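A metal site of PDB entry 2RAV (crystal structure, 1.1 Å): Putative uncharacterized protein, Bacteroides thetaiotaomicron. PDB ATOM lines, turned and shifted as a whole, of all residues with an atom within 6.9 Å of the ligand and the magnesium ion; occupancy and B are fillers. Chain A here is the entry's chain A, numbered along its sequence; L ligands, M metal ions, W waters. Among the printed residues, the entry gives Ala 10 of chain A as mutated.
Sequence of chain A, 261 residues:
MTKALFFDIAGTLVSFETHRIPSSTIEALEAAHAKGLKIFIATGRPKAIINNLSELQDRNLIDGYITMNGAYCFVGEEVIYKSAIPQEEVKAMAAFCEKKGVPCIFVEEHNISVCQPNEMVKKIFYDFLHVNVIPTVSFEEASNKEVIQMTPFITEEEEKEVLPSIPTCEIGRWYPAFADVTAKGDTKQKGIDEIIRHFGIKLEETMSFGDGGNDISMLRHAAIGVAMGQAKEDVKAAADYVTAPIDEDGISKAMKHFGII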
ATOM      1  N   PHE A   7       2.750  21.339  21.386  1.00  0.00           N
ATOM      2  CA  PHE A   7       2.243  20.850  20.115  1.00  0.00           C
ATOM      3  C   PHE A   7       3.138  21.194  18.956  1.00  0.00           C
ATOM      4  O   PHE A   7       3.346  22.369  18.656  1.00  0.00           O
ATOM      5  CB  PHE A   7       0.865  21.456  19.793  1.00  0.00           C
ATOM      6  CG  PHE A   7      -0.223  21.074  20.756  1.00  0.00           C
ATOM      7  CD1 PHE A   7      -0.602  21.873  21.815  1.00  0.00           C
ATOM      8  CD2 PHE A   7      -0.892  19.878  20.578  1.00  0.00           C
ATOM      9  CE1 PHE A   7      -1.581  21.491  22.694  1.00  0.00           C
ATOM     10  CE2 PHE A   7      -1.892  19.496  21.467  1.00  0.00           C
ATOM     11  CZ  PHE A   7      -2.253  20.287  22.511  1.00  0.00           C
ATOM     12  N   ASP A   8       3.615  20.202  18.209  1.00  0.00           N
ATOM     13  CA  ASP A   8       4.105  20.402  16.866  1.00  0.00           C
ATOM     14  C   ASP A   8       2.980  21.001  16.003  1.00  0.00           C
ATOM     15  O   ASP A   8       1.779  20.880  16.325  1.00  0.00           O
ATOM     16  CB  ASP A   8       4.568  19.048  16.312  1.00  0.00           C
ATOM     17  CG  ASP A   8       5.022  19.119  14.881  1.00  0.00           C
ATOM     18  OD1 ASP A   8       5.809  20.031  14.577  1.00  0.00           O
ATOM     19  OD2 ASP A   8       4.506  18.291  14.072  1.00  0.00           O
ATOM     20  N   ILE A   9       3.349  21.636  14.888  1.00  0.00           N
ATOM     21  CA  ILE A   9       2.341  22.185  13.968  1.00  0.00           C
ATOM     22  C   ILE A   9       2.011  21.217  12.847  1.00  0.00           C
ATOM     23  O   ILE A   9       0.923  20.635  12.795  1.00  0.00           O
ATOM     24  CB  ILE A   9       2.672  23.579  13.422  1.00  0.00           C
ATOM     25  CG1 ILE A   9       2.937  24.608  14.528  1.00  0.00           C
ATOM     26  CG2 ILE A   9       1.586  24.019  12.472  1.00  0.00           C
ATOM     27  CD1 ILE A   9       3.503  25.902  14.033  1.00  0.00           C
ATOM     28  N   ALA A  10       2.938  21.040  11.908  1.00  0.00           N
ATOM     29  CA  ALA A  10       2.600  20.301  10.705  1.00  0.00           C
ATOM     30  C   ALA A  10       2.389  18.843  11.009  1.00  0.00           C
ATOM     31  O   ALA A  10       3.237  18.138  11.550  1.00  0.00           O
ATOM     32  CB  ALA A  10       3.768  20.473   9.701  1.00  0.00           C
ATOM     33  N   GLY A  11       1.217  18.331  10.657  1.00  0.00           N
ATOM     34  CA  GLY A  11       0.847  16.955  10.883  1.00  0.00           C
ATOM     35  C   GLY A  11       0.375  16.632  12.288  1.00  0.00           C
ATOM     36  O   GLY A  11       0.014  15.476  12.566  1.00  0.00           O
ATOM     37  N   THR A  12       0.332  17.643  13.143  1.00  0.00           N
ATOM     38  CA  THR A  12      -0.031  17.497  14.559  1.00  0.00           C
ATOM     39  C   THR A  12      -1.212  18.384  14.878  1.00  0.00           C
ATOM     40  O   THR A  12      -2.281  17.902  15.242  1.00  0.00           O
ATOM     41  CB  THR A  12       1.189  17.769  15.456  1.00  0.00           C
ATOM     42  OG1 THR A  12       2.201  16.818  15.112  1.00  0.00           O
ATOM     43  CG2 THR A  12       0.822  17.606  16.895  1.00  0.00           C
ATOM     44  N   PHE A  16      -2.074  17.951   6.704  1.00  0.00           N
ATOM     45  CA  PHE A  16      -1.423  18.117   5.412  1.00  0.00           C
ATOM     46  C   PHE A  16      -2.397  18.090   4.246  1.00  0.00           C
ATOM     47  O   PHE A  16      -2.143  18.585   3.160  1.00  0.00           O
ATOM     48  CB  PHE A  16      -0.532  16.924   5.159  1.00  0.00           C
ATOM     49  CG  PHE A  16       0.685  16.910   6.081  1.00  0.00           C
ATOM     50  CD1 PHE A  16       1.663  17.896   5.913  1.00  0.00           C
ATOM     51  CD2 PHE A  16       0.848  15.986   7.078  1.00  0.00           C
ATOM     52  CE1 PHE A  16       2.793  17.930   6.732  1.00  0.00           C
ATOM     53  CE2 PHE A  16       1.986  15.984   7.872  1.00  0.00           C
ATOM     54  CZ  PHE A  16       2.951  16.961   7.721  1.00  0.00           C
ATOM     55  N   ILE A  41       3.288  26.069  21.388  1.00  0.00           N
ATOM     56  CA  ILE A  41       3.707  25.589  20.095  1.00  0.00           C
ATOM     57  C   ILE A  41       5.143  25.120  20.202  1.00  0.00           C
ATOM     58  O   ILE A  41       5.953  25.784  20.847  1.00  0.00           O
ATOM     59  CB  ILE A  41       3.542  26.721  19.039  1.00  0.00           C
ATOM     60  CG1 ILE A  41       2.067  27.139  18.914  1.00  0.00           C
ATOM     61  CG2 ILE A  41       4.145  26.337  17.708  1.00  0.00           C
ATOM     62  CD1 ILE A  41       1.123  26.066  18.458  1.00  0.00           C
ATOM     63  N   ALA A  42       5.461  24.003  19.536  1.00  0.00           N
ATOM     64  CA  ALA A  42       6.829  23.486  19.484  1.00  0.00           C
ATOM     65  C   ALA A  42       7.094  23.013  18.071  1.00  0.00           C
ATOM     66  O   ALA A  42       6.736  21.881  17.702  1.00  0.00           O
ATOM     67  CB  ALA A  42       7.073  22.378  20.508  1.00  0.00           C
ATOM     68  N   THR A  43       7.677  23.895  17.248  1.00  0.00           N
ATOM     69  CA  THR A  43       7.797  23.670  15.808  1.00  0.00           C
ATOM     70  C   THR A  43       9.209  23.868  15.325  1.00  0.00           C
ATOM     71  O   THR A  43       9.961  24.669  15.876  1.00  0.00           O
ATOM     72  CB  THR A  43       6.825  24.630  15.073  1.00  0.00           C
ATOM     73  OG1 THR A  43       6.855  24.382  13.652  1.00  0.00           O
ATOM     74  CG2 THR A  43       7.121  26.102  15.295  1.00  0.00           C
ATOM     75  N   GLY A  44       9.533  23.170  14.232  1.00  0.00           N
ATOM     76  CA  GLY A  44      10.751  23.442  13.497  1.00  0.00           C
ATOM     77  C   GLY A  44      10.672  24.743  12.756  1.00  0.00           C
ATOM     78  O   GLY A  44      11.710  25.305  12.358  1.00  0.00           O
ATOM     79  N   ARG A  45       9.493  25.272  12.472  1.00  0.00           N
ATOM     80  CA  ARG A  45       9.402  26.480  11.670  1.00  0.00           C
ATOM     81  C   ARG A  45       9.833  27.708  12.486  1.00  0.00           C
ATOM     82  O   ARG A  45       9.600  27.801  13.660  1.00  0.00           O
ATOM     83  CB  ARG A  45       7.976  26.594  11.203  1.00  0.00           C
ATOM     84  CG  ARG A  45       7.467  25.464  10.335  1.00  0.00           C
ATOM     85  CD  ARG A  45       8.401  25.058   9.178  1.00  0.00           C
ATOM     86  NE  ARG A  45       9.009  23.793   9.529  1.00  0.00           N
ATOM     87  CZ  ARG A  45      10.258  23.375   9.442  1.00  0.00           C
ATOM     88  NH1 ARG A  45      11.261  24.184   8.934  1.00  0.00           N
ATOM     89  NH2 ARG A  45      10.334  22.089   9.932  1.00  0.00           N
ATOM     90  N   ASN A  69      12.920  24.629  16.177  1.00  0.00           N
ATOM     91  CA  ASN A  69      13.394  23.430  16.857  1.00  0.00           C
ATOM     92  C   ASN A  69      14.053  23.715  18.214  1.00  0.00           C
ATOM     93  O   ASN A  69      14.920  22.964  18.635  1.00  0.00           O
ATOM     94  CB  ASN A  69      14.377  22.611  15.979  1.00  0.00           C
ATOM     95  CG  ASN A  69      13.586  21.992  14.818  1.00  0.00           C
ATOM     96  OD1 ASN A  69      12.811  21.049  14.987  1.00  0.00           O
ATOM     97  ND2 ASN A  69      13.866  22.556  13.649  1.00  0.00           N
ATOM     98  N   LEU A 129       3.464  22.344   1.653  1.00  0.00           N
ATOM     99  CA  LEU A 129       3.241  22.935   2.984  1.00  0.00           C
ATOM    100  C   LEU A 129       2.601  24.320   2.980  1.00  0.00           C
ATOM    101  O   LEU A 129       2.207  24.914   3.986  1.00  0.00           O
ATOM    102  CB  LEU A 129       4.591  23.023   3.716  1.00  0.00           C
ATOM    103  CG  LEU A 129       5.259  21.690   4.025  1.00  0.00           C
ATOM    104  CD1 LEU A 129       6.650  21.905   4.631  1.00  0.00           C
ATOM    105  CD2 LEU A 129       4.394  20.887   4.962  1.00  0.00           C
ATOM    106  N   TRP A 174      11.891  15.456   9.642  1.00  0.00           N
ATOM    107  CA  TRP A 174      10.673  14.623   9.597  1.00  0.00           C
ATOM    108  C   TRP A 174      10.380  14.212   8.179  1.00  0.00           C
ATOM    109  O   TRP A 174       9.568  13.257   8.032  1.00  0.00           O
ATOM    110  CB  TRP A 174       9.493  15.344  10.207  1.00  0.00           C
ATOM    111  CG  TRP A 174       9.065  16.647   9.574  1.00  0.00           C
ATOM    112  CD1 TRP A 174       9.493  17.883   9.881  1.00  0.00           C
ATOM    113  CD2 TRP A 174       8.091  16.789   8.546  1.00  0.00           C
ATOM    114  NE1 TRP A 174       8.871  18.828   9.102  1.00  0.00           N
ATOM    115  CE2 TRP A 174       7.984  18.166   8.257  1.00  0.00           C
ATOM    116  CE3 TRP A 174       7.288  15.891   7.841  1.00  0.00           C
ATOM    117  CZ2 TRP A 174       7.121  18.650   7.300  1.00  0.00           C
ATOM    118  CZ3 TRP A 174       6.419  16.396   6.860  1.00  0.00           C
ATOM    119  CH2 TRP A 174       6.344  17.767   6.597  1.00  0.00           C
ATOM    120  N   PHE A 178      14.146  17.637   3.108  1.00  0.00           N
ATOM    121  CA  PHE A 178      14.868  18.689   3.776  1.00  0.00           C
ATOM    122  C   PHE A 178      15.081  18.330   5.226  1.00  0.00           C
ATOM    123  O   PHE A 178      14.451  17.428   5.762  1.00  0.00           O
ATOM    124  CB  PHE A 178      14.069  19.993   3.663  1.00  0.00           C
ATOM    125  CG  PHE A 178      12.809  20.039   4.488  1.00  0.00           C
ATOM    126  CD1 PHE A 178      12.758  20.555   5.766  1.00  0.00           C
ATOM    127  CD2 PHE A 178      11.633  19.526   3.922  1.00  0.00           C
ATOM    128  CE1 PHE A 178      11.565  20.571   6.480  1.00  0.00           C
ATOM    129  CE2 PHE A 178      10.426  19.536   4.616  1.00  0.00           C
ATOM    130  CZ  PHE A 178      10.419  20.066   5.874  1.00  0.00           C
ATOM    131  N   ASP A 180      16.203  20.484   9.146  1.00  0.00           N
ATOM    132  CA  ASP A 180      16.429  21.680   9.880  1.00  0.00           C
ATOM    133  C   ASP A 180      17.693  21.592  10.756  1.00  0.00           C
ATOM    134  O   ASP A 180      17.826  20.628  11.517  1.00  0.00           O
ATOM    135  CB  ASP A 180      15.243  22.012  10.779  1.00  0.00           C
ATOM    136  CG  ASP A 180      13.918  22.296  10.102  1.00  0.00           C
ATOM    137  OD1 ASP A 180      13.907  23.006   9.070  1.00  0.00           O
ATOM    138  OD2 ASP A 180      12.894  21.791  10.606  1.00  0.00           O
ATOM    139  N   LYS A 188      13.616  20.411  20.163  1.00  0.00           N
ATOM    140  CA  LYS A 188      12.406  20.776  20.882  1.00  0.00           C
ATOM    141  C   LYS A 188      12.465  20.418  22.369  1.00  0.00           C
ATOM    142  O   LYS A 188      11.770  21.070  23.157  1.00  0.00           O
ATOM    143  CB  LYS A 188      11.172  20.134  20.222  1.00  0.00           C
ATOM    144  CG  LYS A 188      10.897  20.658  18.810  1.00  0.00           C
ATOM    145  CD  LYS A 188       9.664  20.048  18.175  1.00  0.00           C
ATOM    146  CE  LYS A 188       9.539  20.454  16.725  1.00  0.00           C
ATOM    147  NZ  LYS A 188       8.249  20.055  16.137  1.00  0.00           N
ATOM    148  N   GLY A 210       3.356  15.078  18.686  1.00  0.00           N
ATOM    149  CA  GLY A 210       4.094  15.205  17.454  1.00  0.00           C
ATOM    150  C   GLY A 210       3.838  14.067  16.495  1.00  0.00           C
ATOM    151  O   GLY A 210       3.282  13.042  16.852  1.00  0.00           O
ATOM    152  N   ASP A 211       4.237  14.323  15.242  1.00  0.00           N
ATOM    153  CA  ASP A 211       4.093  13.362  14.194  1.00  0.00           C
ATOM    154  C   ASP A 211       5.397  12.993  13.487  1.00  0.00           C
ATOM    155  O   ASP A 211       5.327  12.126  12.620  1.00  0.00           O
ATOM    156  CB  ASP A 211       3.114  13.845  13.091  1.00  0.00           C
ATOM    157  CG  ASP A 211       3.733  14.920  12.229  1.00  0.00           C
ATOM    158  OD1 ASP A 211       4.362  15.824  12.824  1.00  0.00           O
ATOM    159  OD2 ASP A 211       3.608  14.877  10.973  1.00  0.00           O
ATOM    160  N   GLY A 212       6.490  13.630  13.819  1.00  0.00           N
ATOM    161  CA  GLY A 212       7.676  13.589  12.973  1.00  0.00           C
ATOM    162  C   GLY A 212       8.959  13.299  13.676  1.00  0.00           C
ATOM    163  O   GLY A 212       9.071  13.381  14.872  1.00  0.00           O
ATOM    164  N   GLY A 213       9.994  13.001  12.854  1.00  0.00           N
ATOM    165  CA  GLY A 213      11.284  12.692  13.445  1.00  0.00           C
ATOM    166  C   GLY A 213      11.886  13.781  14.322  1.00  0.00           C
ATOM    167  O   GLY A 213      12.593  13.506  15.272  1.00  0.00           O
ATOM    168  N   ASN A 214      11.560  15.038  13.984  1.00  0.00           N
ATOM    169  CA  ASN A 214      12.059  16.152  14.777  1.00  0.00           C
ATOM    170  C   ASN A 214      11.317  16.366  16.085  1.00  0.00           C
ATOM    171  O   ASN A 214      11.662  17.262  16.854  1.00  0.00           O
ATOM    172  CB  ASN A 214      12.106  17.440  13.944  1.00  0.00           C
ATOM    173  CG  ASN A 214      10.780  17.992  13.566  1.00  0.00           C
ATOM    174  OD1 ASN A 214       9.848  17.227  13.253  1.00  0.00           O
ATOM    175  ND2 ASN A 214      10.624  19.312  13.554  1.00  0.00           N
ATOM    176  N   ASP A 215      10.310  15.504  16.328  1.00  0.00           N
ATOM    177  CA  ASP A 215       9.568  15.458  17.594  1.00  0.00           C
ATOM    178  C   ASP A 215      10.098  14.378  18.534  1.00  0.00           C
ATOM    179  O   ASP A 215       9.640  14.327  19.691  1.00  0.00           O
ATOM    180  CB  ASP A 215       8.067  15.220  17.318  1.00  0.00           C
ATOM    181  CG  ASP A 215       7.497  16.317  16.459  1.00  0.00           C
ATOM    182  OD1 ASP A 215       7.765  17.486  16.741  1.00  0.00           O
ATOM    183  OD2 ASP A 215       6.733  15.939  15.518  1.00  0.00           O
HETATM  184  W1  LIG L   1       6.835  20.918  12.311  1.00  0.00           W
HETATM  185  O1  LIG L   1       8.153  20.880  13.433  1.00  0.00           O
HETATM  186  O2  LIG L   1       6.118  19.410  11.795  1.00  0.00           O
HETATM  187  O3  LIG L   1       7.571  21.524  10.881  1.00  0.00           O
HETATM  188  O4  LIG L   1       5.669  22.104  12.716  1.00  0.00           O
HETATM  189 MG    MG M   1       5.178  17.666  12.260  1.00  0.00          MG
HETATM  190  O   HOH W   1       4.634  23.893  10.440  1.00  0.00           O
HETATM  191  O   HOH W   2       5.479  16.880  10.371  1.00  0.00           O
HETATM  192  O   HOH W   3       6.982  16.935  13.059  1.00  0.00           O
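Within 4 Å of the magnesium ion: Asp 8, Ala 10 and Asp 211.
N of Ile 9 lies close to O4 of the ligand, 3.2 Å away. The backbone NH of Gly 44 lies close to an oxygen (O1) of the ligand (2.8 Å). NH2 of Arg 45 sits close to O3 of the ligand (3.0 Å). The indole nitrogen (NE1) of Trp 174 sits close to an oxygen (O3) of the ligand (3.5 Å). An oxygen (O1) of the ligand sits close to the side-chain amino group (NZ) of Lys 188, 2.8 Å away. The side-chain amide nitrogen (ND2) of Asn 214 sits close to an oxygen (O1) of the ligand (2.9 Å). Hydrophobic or aromatic side chains within 4 Å of the ligand: Ile 9 and Ala 10. Along chain A the residues within 4 Å of the ligand span positions 8 to 214. The nearest printed residue that does not touch the ligand is Asp 211 (4.1 Å).
The magnesium ion is bound by the side-chain carboxylate (OD2) of Asp 8 (2.0 Å), an oxygen (O2) of the ligand (2.0 Å), water W2 (2.1 Å), the side-chain carboxylate (OD1) of Asp 211 (2.1 Å), water W3 (2.1 Å) and the backbone carbonyl oxygen (O) of Ala 10 (2.1 Å).
The side-chain hydroxyl (OG1) of Thr 43 lies close to an oxygen (O4) of the ligand (2.7 Å).
Water W3 lies within hydrogen-bond range of the side-chain carboxylate of Asp 215 (2.7 Å), the side-chain amide oxygen of Asn 214 (2.9 Å) and the backbone NH of Gly 212 (3.4 Å).
OD2 of Asp 8 lies close to OG1 of Thr 12 (2.9 Å). N of Asp 211 sits at hydrogen-bond distance from OD2 of Asp 215, 3.0 Å away. The backbone NH of Asp 211 lies within hydrogen-bond range of the side-chain hydroxyl of Thr 12, at 3.2 Å. The side-chain hydroxyl (OG1) of Thr 43 is in hydrogen-bond range of the backbone NH (N) of Arg 45 (3.0 Å). The side-chain carboxylate of Asp 215 is in salt-bridge range of the side-chain amino group of Lys 188. The side-chain amino group of Lys 188 sits at hydrogen-bond distance from the backbone carbonyl oxygen of Ala 42 (2.8 Å). N of Lys 188 sits at hydrogen-bond distance from O of Asn 69. ND2 of Asn 214 is in hydrogen-bond range of OD1 of Asn 69.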
